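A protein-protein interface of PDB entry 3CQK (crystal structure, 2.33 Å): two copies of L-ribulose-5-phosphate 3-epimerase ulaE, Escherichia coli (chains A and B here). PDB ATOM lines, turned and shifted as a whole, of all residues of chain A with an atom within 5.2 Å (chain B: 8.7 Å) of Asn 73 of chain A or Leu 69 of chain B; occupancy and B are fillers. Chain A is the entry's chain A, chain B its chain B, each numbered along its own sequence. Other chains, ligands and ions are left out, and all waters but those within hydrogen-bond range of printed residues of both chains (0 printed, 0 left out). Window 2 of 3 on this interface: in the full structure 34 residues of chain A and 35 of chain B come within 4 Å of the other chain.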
ATOM      1  N   LEU A  69     -19.999  34.001  34.907  1.00  0.00           N
ATOM      2  CA  LEU A  69     -19.137  33.541  33.808  1.00  0.00           C
ATOM      3  C   LEU A  69     -17.671  33.848  34.026  1.00  0.00           C
ATOM      4  O   LEU A  69     -16.810  33.146  33.481  1.00  0.00           O
ATOM      5  CB  LEU A  69     -19.609  34.057  32.453  1.00  0.00           C
ATOM      6  CG  LEU A  69     -20.979  33.536  31.996  1.00  0.00           C
ATOM      7  CD1 LEU A  69     -21.455  34.196  30.697  1.00  0.00           C
ATOM      8  CD2 LEU A  69     -21.018  31.989  31.873  1.00  0.00           C
ATOM      9  N   ALA A  70     -17.381  34.869  34.827  1.00  0.00           N
ATOM     10  CA  ALA A  70     -16.006  35.179  35.205  1.00  0.00           C
ATOM     11  C   ALA A  70     -15.412  34.098  36.119  1.00  0.00           C
ATOM     12  O   ALA A  70     -14.274  33.703  35.928  1.00  0.00           O
ATOM     13  CB  ALA A  70     -15.905  36.591  35.856  1.00  0.00           C
ATOM     14  N   LEU A  71     -16.172  33.615  37.102  1.00  0.00           N
ATOM     15  CA  LEU A  71     -15.742  32.435  37.893  1.00  0.00           C
ATOM     16  C   LEU A  71     -15.505  31.200  37.022  1.00  0.00           C
ATOM     17  O   LEU A  71     -14.482  30.526  37.167  1.00  0.00           O
ATOM     18  CB  LEU A  71     -16.762  32.099  39.009  1.00  0.00           C
ATOM     19  CG  LEU A  71     -16.480  30.930  39.957  1.00  0.00           C
ATOM     20  CD1 LEU A  71     -15.122  31.073  40.649  1.00  0.00           C
ATOM     21  CD2 LEU A  71     -17.589  30.793  40.997  1.00  0.00           C
ATOM     22  N   VAL A  72     -16.435  30.890  36.122  1.00  0.00           N
ATOM     23  CA  VAL A  72     -16.236  29.750  35.210  1.00  0.00           C
ATOM     24  C   VAL A  72     -14.923  29.915  34.432  1.00  0.00           C
ATOM     25  O   VAL A  72     -14.144  28.966  34.301  1.00  0.00           O
ATOM     26  CB  VAL A  72     -17.428  29.577  34.227  1.00  0.00           C
ATOM     27  CG1 VAL A  72     -17.148  28.476  33.192  1.00  0.00           C
ATOM     28  CG2 VAL A  72     -18.712  29.255  34.982  1.00  0.00           C
ATOM     29  N   ASN A  73     -14.675  31.141  33.946  1.00  0.00           N
ATOM     30  CA  ASN A  73     -13.438  31.481  33.230  1.00  0.00           C
ATOM     31  C   ASN A  73     -12.182  31.168  34.047  1.00  0.00           C
ATOM     32  O   ASN A  73     -11.293  30.507  33.534  1.00  0.00           O
ATOM     33  CB  ASN A  73     -13.445  32.965  32.833  1.00  0.00           C
ATOM     34  CG  ASN A  73     -12.878  33.206  31.477  1.00  0.00           C
ATOM     35  OD1 ASN A  73     -11.658  33.308  31.305  1.00  0.00           O
ATOM     36  ND2 ASN A  73     -13.754  33.303  30.482  1.00  0.00           N
ATOM     37  N   ALA A  74     -12.113  31.644  35.298  1.00  0.00           N
ATOM     38  CA  ALA A  74     -10.943  31.432  36.170  1.00  0.00           C
ATOM     39  C   ALA A  74     -10.694  29.955  36.481  1.00  0.00           C
ATOM     40  O   ALA A  74      -9.546  29.514  36.516  1.00  0.00           O
ATOM     41  CB  ALA A  74     -11.093  32.201  37.467  1.00  0.00           C
ATOM     42  N   ILE A  75     -11.774  29.211  36.712  1.00  0.00           N
ATOM     43  CA  ILE A  75     -11.720  27.763  36.892  1.00  0.00           C
ATOM     44  C   ILE A  75     -11.081  27.053  35.698  1.00  0.00           C
ATOM     45  O   ILE A  75     -10.136  26.266  35.858  1.00  0.00           O
ATOM     46  CB  ILE A  75     -13.133  27.180  37.178  1.00  0.00           C
ATOM     47  CG1 ILE A  75     -13.635  27.642  38.558  1.00  0.00           C
ATOM     48  CG2 ILE A  75     -13.141  25.630  37.033  1.00  0.00           C
ATOM     49  CD1 ILE A  75     -15.125  27.415  38.807  1.00  0.00           C
ATOM     50  N   VAL A  76     -11.601  27.333  34.501  1.00  0.00           N
ATOM     51  CA  VAL A  76     -11.193  26.614  33.274  1.00  0.00           C
ATOM     52  C   VAL A  76      -9.738  26.934  32.944  1.00  0.00           C
ATOM     53  O   VAL A  76      -8.985  26.078  32.491  1.00  0.00           O
ATOM     54  CB  VAL A  76     -12.158  26.918  32.095  1.00  0.00           C
ATOM     55  CG1 VAL A  76     -11.566  26.484  30.741  1.00  0.00           C
ATOM     56  CG2 VAL A  76     -13.490  26.216  32.314  1.00  0.00           C
ATOM     57  N   GLU A  77      -9.352  28.167  33.233  1.00  0.00           N
ATOM     58  CA  GLU A  77      -8.041  28.712  32.962  1.00  0.00           C
ATOM     59  C   GLU A  77      -6.933  28.252  33.936  1.00  0.00           C
ATOM     60  O   GLU A  77      -5.809  27.972  33.506  1.00  0.00           O
ATOM     61  CB  GLU A  77      -8.215  30.223  32.945  1.00  0.00           C
ATOM     62  CG  GLU A  77      -7.035  31.099  33.238  1.00  0.00           C
ATOM     63  CD  GLU A  77      -7.363  32.559  32.904  1.00  0.00           C
ATOM     64  OE1 GLU A  77      -8.186  32.789  31.958  1.00  0.00           O
ATOM     65  OE2 GLU A  77      -6.805  33.471  33.575  1.00  0.00           O
ATOM     66  N   THR A  78      -7.235  28.168  35.233  1.00  0.00           N
ATOM     67  CA  THR A  78      -6.259  27.682  36.219  1.00  0.00           C
ATOM     68  C   THR A  78      -6.230  26.161  36.331  1.00  0.00           C
ATOM     69  O   THR A  78      -5.194  25.589  36.698  1.00  0.00           O
ATOM     70  CB  THR A  78      -6.525  28.231  37.624  1.00  0.00           C
ATOM     71  OG1 THR A  78      -7.854  27.879  38.017  1.00  0.00           O
ATOM     72  CG2 THR A  78      -6.373  29.735  37.653  1.00  0.00           C
ATOM     73  N   TRP B  63     -12.384  19.651  22.279  1.00  0.00           N
ATOM     74  CA  TRP B  63     -12.569  21.098  22.218  1.00  0.00           C
ATOM     75  C   TRP B  63     -11.535  21.822  23.083  1.00  0.00           C
ATOM     76  O   TRP B  63     -11.005  21.267  24.044  1.00  0.00           O
ATOM     77  CB  TRP B  63     -13.959  21.503  22.699  1.00  0.00           C
ATOM     78  CG  TRP B  63     -15.078  21.441  21.685  1.00  0.00           C
ATOM     79  CD1 TRP B  63     -14.999  21.095  20.347  1.00  0.00           C
ATOM     80  CD2 TRP B  63     -16.451  21.786  21.925  1.00  0.00           C
ATOM     81  NE1 TRP B  63     -16.248  21.165  19.769  1.00  0.00           N
ATOM     82  CE2 TRP B  63     -17.151  21.600  20.707  1.00  0.00           C
ATOM     83  CE3 TRP B  63     -17.157  22.242  23.053  1.00  0.00           C
ATOM     84  CZ2 TRP B  63     -18.520  21.848  20.588  1.00  0.00           C
ATOM     85  CZ3 TRP B  63     -18.512  22.484  22.934  1.00  0.00           C
ATOM     86  CH2 TRP B  63     -19.183  22.289  21.700  1.00  0.00           C
ATOM     87  N   SER B  64     -11.261  23.069  22.720  1.00  0.00           N
ATOM     88  CA  SER B  64     -10.357  23.931  23.451  1.00  0.00           C
ATOM     89  C   SER B  64     -11.108  24.597  24.599  1.00  0.00           C
ATOM     90  O   SER B  64     -12.338  24.628  24.617  1.00  0.00           O
ATOM     91  CB  SER B  64      -9.819  25.003  22.492  1.00  0.00           C
ATOM     92  OG  SER B  64     -10.881  25.829  22.051  1.00  0.00           O
ATOM     93  N   ARG B  65     -10.370  25.174  25.543  1.00  0.00           N
ATOM     94  CA  ARG B  65     -11.003  25.881  26.661  1.00  0.00           C
ATOM     95  C   ARG B  65     -12.000  26.937  26.182  1.00  0.00           C
ATOM     96  O   ARG B  65     -13.082  27.069  26.757  1.00  0.00           O
ATOM     97  CB  ARG B  65      -9.950  26.502  27.568  1.00  0.00           C
ATOM     98  CG  ARG B  65      -9.019  25.477  28.223  1.00  0.00           C
ATOM     99  CD  ARG B  65      -8.054  26.183  29.168  1.00  0.00           C
ATOM    100  NE  ARG B  65      -6.774  25.488  29.254  1.00  0.00           N
ATOM    101  CZ  ARG B  65      -5.737  25.732  28.457  1.00  0.00           C
ATOM    102  NH1 ARG B  65      -5.820  26.656  27.501  1.00  0.00           N
ATOM    103  NH2 ARG B  65      -4.611  25.042  28.605  1.00  0.00           N
ATOM    104  N   GLU B  66     -11.636  27.655  25.115  1.00  0.00           N
ATOM    105  CA  GLU B  66     -12.479  28.673  24.461  1.00  0.00           C
ATOM    106  C   GLU B  66     -13.798  28.158  23.868  1.00  0.00           C
ATOM    107  O   GLU B  66     -14.826  28.836  23.954  1.00  0.00           O
ATOM    108  CB  GLU B  66     -11.682  29.398  23.365  1.00  0.00           C
ATOM    109  CG  GLU B  66     -10.612  30.366  23.899  1.00  0.00           C
ATOM    110  CD  GLU B  66      -9.354  29.656  24.425  1.00  0.00           C
ATOM    111  OE1 GLU B  66      -9.102  28.476  24.025  1.00  0.00           O
ATOM    112  OE2 GLU B  66      -8.622  30.296  25.235  1.00  0.00           O
ATOM    113  N   GLN B  67     -13.749  26.984  23.236  1.00  0.00           N
ATOM    114  CA  GLN B  67     -14.934  26.331  22.697  1.00  0.00           C
ATOM    115  C   GLN B  67     -15.874  25.909  23.818  1.00  0.00           C
ATOM    116  O   GLN B  67     -17.081  26.141  23.736  1.00  0.00           O
ATOM    117  CB  GLN B  67     -14.547  25.131  21.823  1.00  0.00           C
ATOM    118  CG  GLN B  67     -13.858  25.540  20.530  1.00  0.00           C
ATOM    119  CD  GLN B  67     -13.483  24.369  19.648  1.00  0.00           C
ATOM    120  OE1 GLN B  67     -14.194  24.065  18.681  1.00  0.00           O
ATOM    121  NE2 GLN B  67     -12.379  23.695  19.978  1.00  0.00           N
ATOM    122  N   ARG B  68     -15.303  25.318  24.870  1.00  0.00           N
ATOM    123  CA  ARG B  68     -16.051  24.924  26.077  1.00  0.00           C
ATOM    124  C   ARG B  68     -16.681  26.140  26.771  1.00  0.00           C
ATOM    125  O   ARG B  68     -17.859  26.133  27.119  1.00  0.00           O
ATOM    126  CB  ARG B  68     -15.132  24.162  27.039  1.00  0.00           C
ATOM    127  CG  ARG B  68     -14.648  22.829  26.468  1.00  0.00           C
ATOM    128  CD  ARG B  68     -13.407  22.317  27.183  1.00  0.00           C
ATOM    129  NE  ARG B  68     -12.791  21.255  26.403  1.00  0.00           N
ATOM    130  CZ  ARG B  68     -12.697  19.981  26.769  1.00  0.00           C
ATOM    131  NH1 ARG B  68     -12.123  19.111  25.936  1.00  0.00           N
ATOM    132  NH2 ARG B  68     -13.154  19.567  27.954  1.00  0.00           N
ATOM    133  N   LEU B  69     -15.909  27.205  26.929  1.00  0.00           N
ATOM    134  CA  LEU B  69     -16.448  28.430  27.503  1.00  0.00           C
ATOM    135  C   LEU B  69     -17.563  29.051  26.645  1.00  0.00           C
ATOM    136  O   LEU B  69     -18.535  29.554  27.203  1.00  0.00           O
ATOM    137  CB  LEU B  69     -15.323  29.444  27.817  1.00  0.00           C
ATOM    138  CG  LEU B  69     -14.323  29.028  28.928  1.00  0.00           C
ATOM    139  CD1 LEU B  69     -12.944  29.790  28.841  1.00  0.00           C
ATOM    140  CD2 LEU B  69     -14.936  29.161  30.316  1.00  0.00           C
ATOM    141  N   ALA B  70     -17.434  29.014  25.313  1.00  0.00           N
ATOM    142  CA  ALA B  70     -18.459  29.591  24.408  1.00  0.00           C
ATOM    143  C   ALA B  70     -19.813  28.895  24.564  1.00  0.00           C
ATOM    144  O   ALA B  70     -20.860  29.539  24.493  1.00  0.00           O
ATOM    145  CB  ALA B  70     -17.997  29.550  22.943  1.00  0.00           C
ATOM    146  N   LEU B  71     -19.776  27.582  24.796  1.00  0.00           N
ATOM    147  CA  LEU B  71     -20.968  26.785  25.113  1.00  0.00           C
ATOM    148  C   LEU B  71     -21.586  27.198  26.457  1.00  0.00           C
ATOM    149  O   LEU B  71     -22.783  27.449  26.538  1.00  0.00           O
ATOM    150  CB  LEU B  71     -20.664  25.267  25.061  1.00  0.00           C
ATOM    151  CG  LEU B  71     -21.837  24.346  25.467  1.00  0.00           C
ATOM    152  CD1 LEU B  71     -23.076  24.591  24.601  1.00  0.00           C
ATOM    153  CD2 LEU B  71     -21.466  22.872  25.421  1.00  0.00           C
ATOM    154  N   VAL B  72     -20.781  27.266  27.509  1.00  0.00           N
ATOM    155  CA  VAL B  72     -21.263  27.800  28.791  1.00  0.00           C
ATOM    156  C   VAL B  72     -21.908  29.195  28.642  1.00  0.00           C
ATOM    157  O   VAL B  72     -23.002  29.445  29.158  1.00  0.00           O
ATOM    158  CB  VAL B  72     -20.142  27.829  29.872  1.00  0.00           C
ATOM    159  CG1 VAL B  72     -20.690  28.320  31.227  1.00  0.00           C
ATOM    160  CG2 VAL B  72     -19.510  26.445  30.014  1.00  0.00           C
ATOM    161  N   ASN B  73     -21.232  30.094  27.928  1.00  0.00           N
ATOM    162  CA  ASN B  73     -21.769  31.428  27.670  1.00  0.00           C
ATOM    163  C   ASN B  73     -23.160  31.405  27.061  1.00  0.00           C
ATOM    164  O   ASN B  73     -24.030  32.152  27.507  1.00  0.00           O
ATOM    165  CB  ASN B  73     -20.834  32.244  26.771  1.00  0.00           C
ATOM    166  CG  ASN B  73     -19.500  32.545  27.431  1.00  0.00           C
ATOM    167  OD1 ASN B  73     -19.298  32.256  28.611  1.00  0.00           O
ATOM    168  ND2 ASN B  73     -18.571  33.109  26.660  1.00  0.00           N
ATOM    169  N   ALA B  74     -23.358  30.545  26.052  1.00  0.00           N
ATOM    170  CA  ALA B  74     -24.633  30.419  25.344  1.00  0.00           C
ATOM    171  C   ALA B  74     -25.765  29.859  26.227  1.00  0.00           C
ATOM    172  O   ALA B  74     -26.915  30.308  26.139  1.00  0.00           O
ATOM    173  CB  ALA B  74     -24.451  29.555  24.100  1.00  0.00           C
ATOM    174  N   ILE B  75     -25.428  28.870  27.055  1.00  0.00           N
ATOM    175  CA  ILE B  75     -26.360  28.282  28.029  1.00  0.00           C
ATOM    176  C   ILE B  75     -26.864  29.335  29.021  1.00  0.00           C
ATOM    177  O   ILE B  75     -28.070  29.480  29.248  1.00  0.00           O
ATOM    178  CB  ILE B  75     -25.685  27.088  28.806  1.00  0.00           C
ATOM    179  CG1 ILE B  75     -25.508  25.870  27.887  1.00  0.00           C
ATOM    180  CG2 ILE B  75     -26.462  26.735  30.101  1.00  0.00           C
ATOM    181  CD1 ILE B  75     -24.430  24.883  28.368  1.00  0.00           C
ATOM    182  N   VAL B  76     -25.920  30.052  29.618  1.00  0.00           N
ATOM    183  CA  VAL B  76     -26.222  31.134  30.551  1.00  0.00           C
ATOM    184  C   VAL B  76     -27.004  32.287  29.871  1.00  0.00           C
ATOM    185  O   VAL B  76     -28.009  32.758  30.416  1.00  0.00           O
ATOM    186  CB  VAL B  76     -24.918  31.589  31.284  1.00  0.00           C
ATOM    187  CG1 VAL B  76     -25.087  32.934  31.993  1.00  0.00           C
ATOM    188  CG2 VAL B  76     -24.465  30.510  32.267  1.00  0.00           C
ATOM    189  N   PHE B 116     -14.954  16.880  30.173  1.00  0.00           N
ATOM    190  CA  PHE B 116     -15.852  17.740  29.398  1.00  0.00           C
ATOM    191  C   PHE B 116     -17.075  18.132  30.224  1.00  0.00           C
ATOM    192  O   PHE B 116     -17.452  19.304  30.264  1.00  0.00           O
ATOM    193  CB  PHE B 116     -16.282  17.050  28.109  1.00  0.00           C
ATOM    194  CG  PHE B 116     -17.013  17.957  27.131  1.00  0.00           C
ATOM    195  CD1 PHE B 116     -16.313  18.628  26.124  1.00  0.00           C
ATOM    196  CD2 PHE B 116     -18.397  18.102  27.193  1.00  0.00           C
ATOM    197  CE1 PHE B 116     -16.982  19.436  25.206  1.00  0.00           C
ATOM    198  CE2 PHE B 116     -19.072  18.930  26.281  1.00  0.00           C
ATOM    199  CZ  PHE B 116     -18.372  19.588  25.283  1.00  0.00           C
ATOM    200  N   ASP B 119     -15.821  20.764  32.880  1.00  0.00           N
ATOM    201  CA  ASP B 119     -15.583  22.043  32.193  1.00  0.00           C
ATOM    202  C   ASP B 119     -16.849  22.800  31.813  1.00  0.00           C
ATOM    203  O   ASP B 119     -16.930  24.034  31.984  1.00  0.00           O
ATOM    204  CB  ASP B 119     -14.740  21.837  30.921  1.00  0.00           C
ATOM    205  CG  ASP B 119     -13.301  21.476  31.222  1.00  0.00           C
ATOM    206  OD1 ASP B 119     -12.816  21.694  32.364  1.00  0.00           O
ATOM    207  OD2 ASP B 119     -12.635  20.970  30.290  1.00  0.00           O
ATOM    208  N   VAL B 120     -17.831  22.062  31.304  1.00  0.00           N
ATOM    209  CA  VAL B 120     -19.046  22.666  30.754  1.00  0.00           C
ATOM    210  C   VAL B 120     -20.272  22.617  31.657  1.00  0.00           C
ATOM    211  O   VAL B 120     -21.276  23.270  31.358  1.00  0.00           O
ATOM    212  CB  VAL B 120     -19.383  22.093  29.353  1.00  0.00           C
ATOM    213  CG1 VAL B 120     -20.772  22.497  28.945  1.00  0.00           C
ATOM    214  CG2 VAL B 120     -18.395  22.634  28.330  1.00  0.00           C
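OD1 of Asn 73 of chain B sits close to O of Leu 69 of chain B.
Val 72 of chain B touches Leu 69 of chain A (CG1 to CD2, 3.7 Å). Asn 73 of chain B touches Leu 69 of chain A (OD1 to CD1, 3.6 Å). CD2 of Leu 69 of chain A touches CG2 of Val 76 of chain B, 3.8 Å away. Val 72 of chain A touches Leu 69 of chain B. Asn 73 of chain A touches Leu 69 of chain B (ND2 to CD1, 3.96 Å). O of Val 76 of chain A touches CD of Arg 65 of chain B, 3.5 Å away. Leu 69 of chain B touches Val 76 of chain A (CD2 to CG2, 3.8 Å).
Asn 73 of chain A touches one residue of chain B. Of chain A, only Val 72, Asn 73 and Val 76 come within 4 Å of Leu 69 of chain B. Of the printed residues of chain B, Val 72 of chain A touches Leu 69. No residue of chain B comes within 4 Å of Ala 74 of chain A. Of the printed residues of chain A, Val 76 of chain B touches Leu 69 (3.8 Å). Of the printed residues of chain A, Arg 65 of chain B touches Val 76 (3.5 Å). Of the printed residues of chain A, Asn 73 of chain B touches Leu 69 (3.6 Å). Printed residues of chain B within 4 Å of Val 76 of chain A: Arg 65 (3.5 Å) and Leu 69 (3.8 Å). Gln 67 of chain B touches none of the printed residues of chain A. The nearest residue of chain B that does not touch Asn 73 of chain A is Asn 73 of chain B (5.9 Å).
Of the 10 printed residues of chain A, 4 touch a printed residue of chain B. Printed residues of chain B that touch a printed residue of chain A: Arg 65, Leu 69, Val 72, Asn 73 and Val 76. Hydrophobic or aromatic side chains of chain B within 4 Å of the printed part of chain A: Leu 69, Val 72 and Val 76.
Leu 69 of chain A touches Val 72 of chain B, and with the chains exchanged Val 72 of chain A touches Leu 69 of chain B. Leu 69 of chain A touches Asn 73 of chain B, and with the chains exchanged Asn 73 of chain A touches Leu 69 of chain B. Leu 69 of chain A touches Val 76 of chain B, and with the chains exchanged Val 76 of chain A touches Leu 69 of chain B. Positions printed for both chains: 69, 70, 71, 72, 73, 74, 75 and 76.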
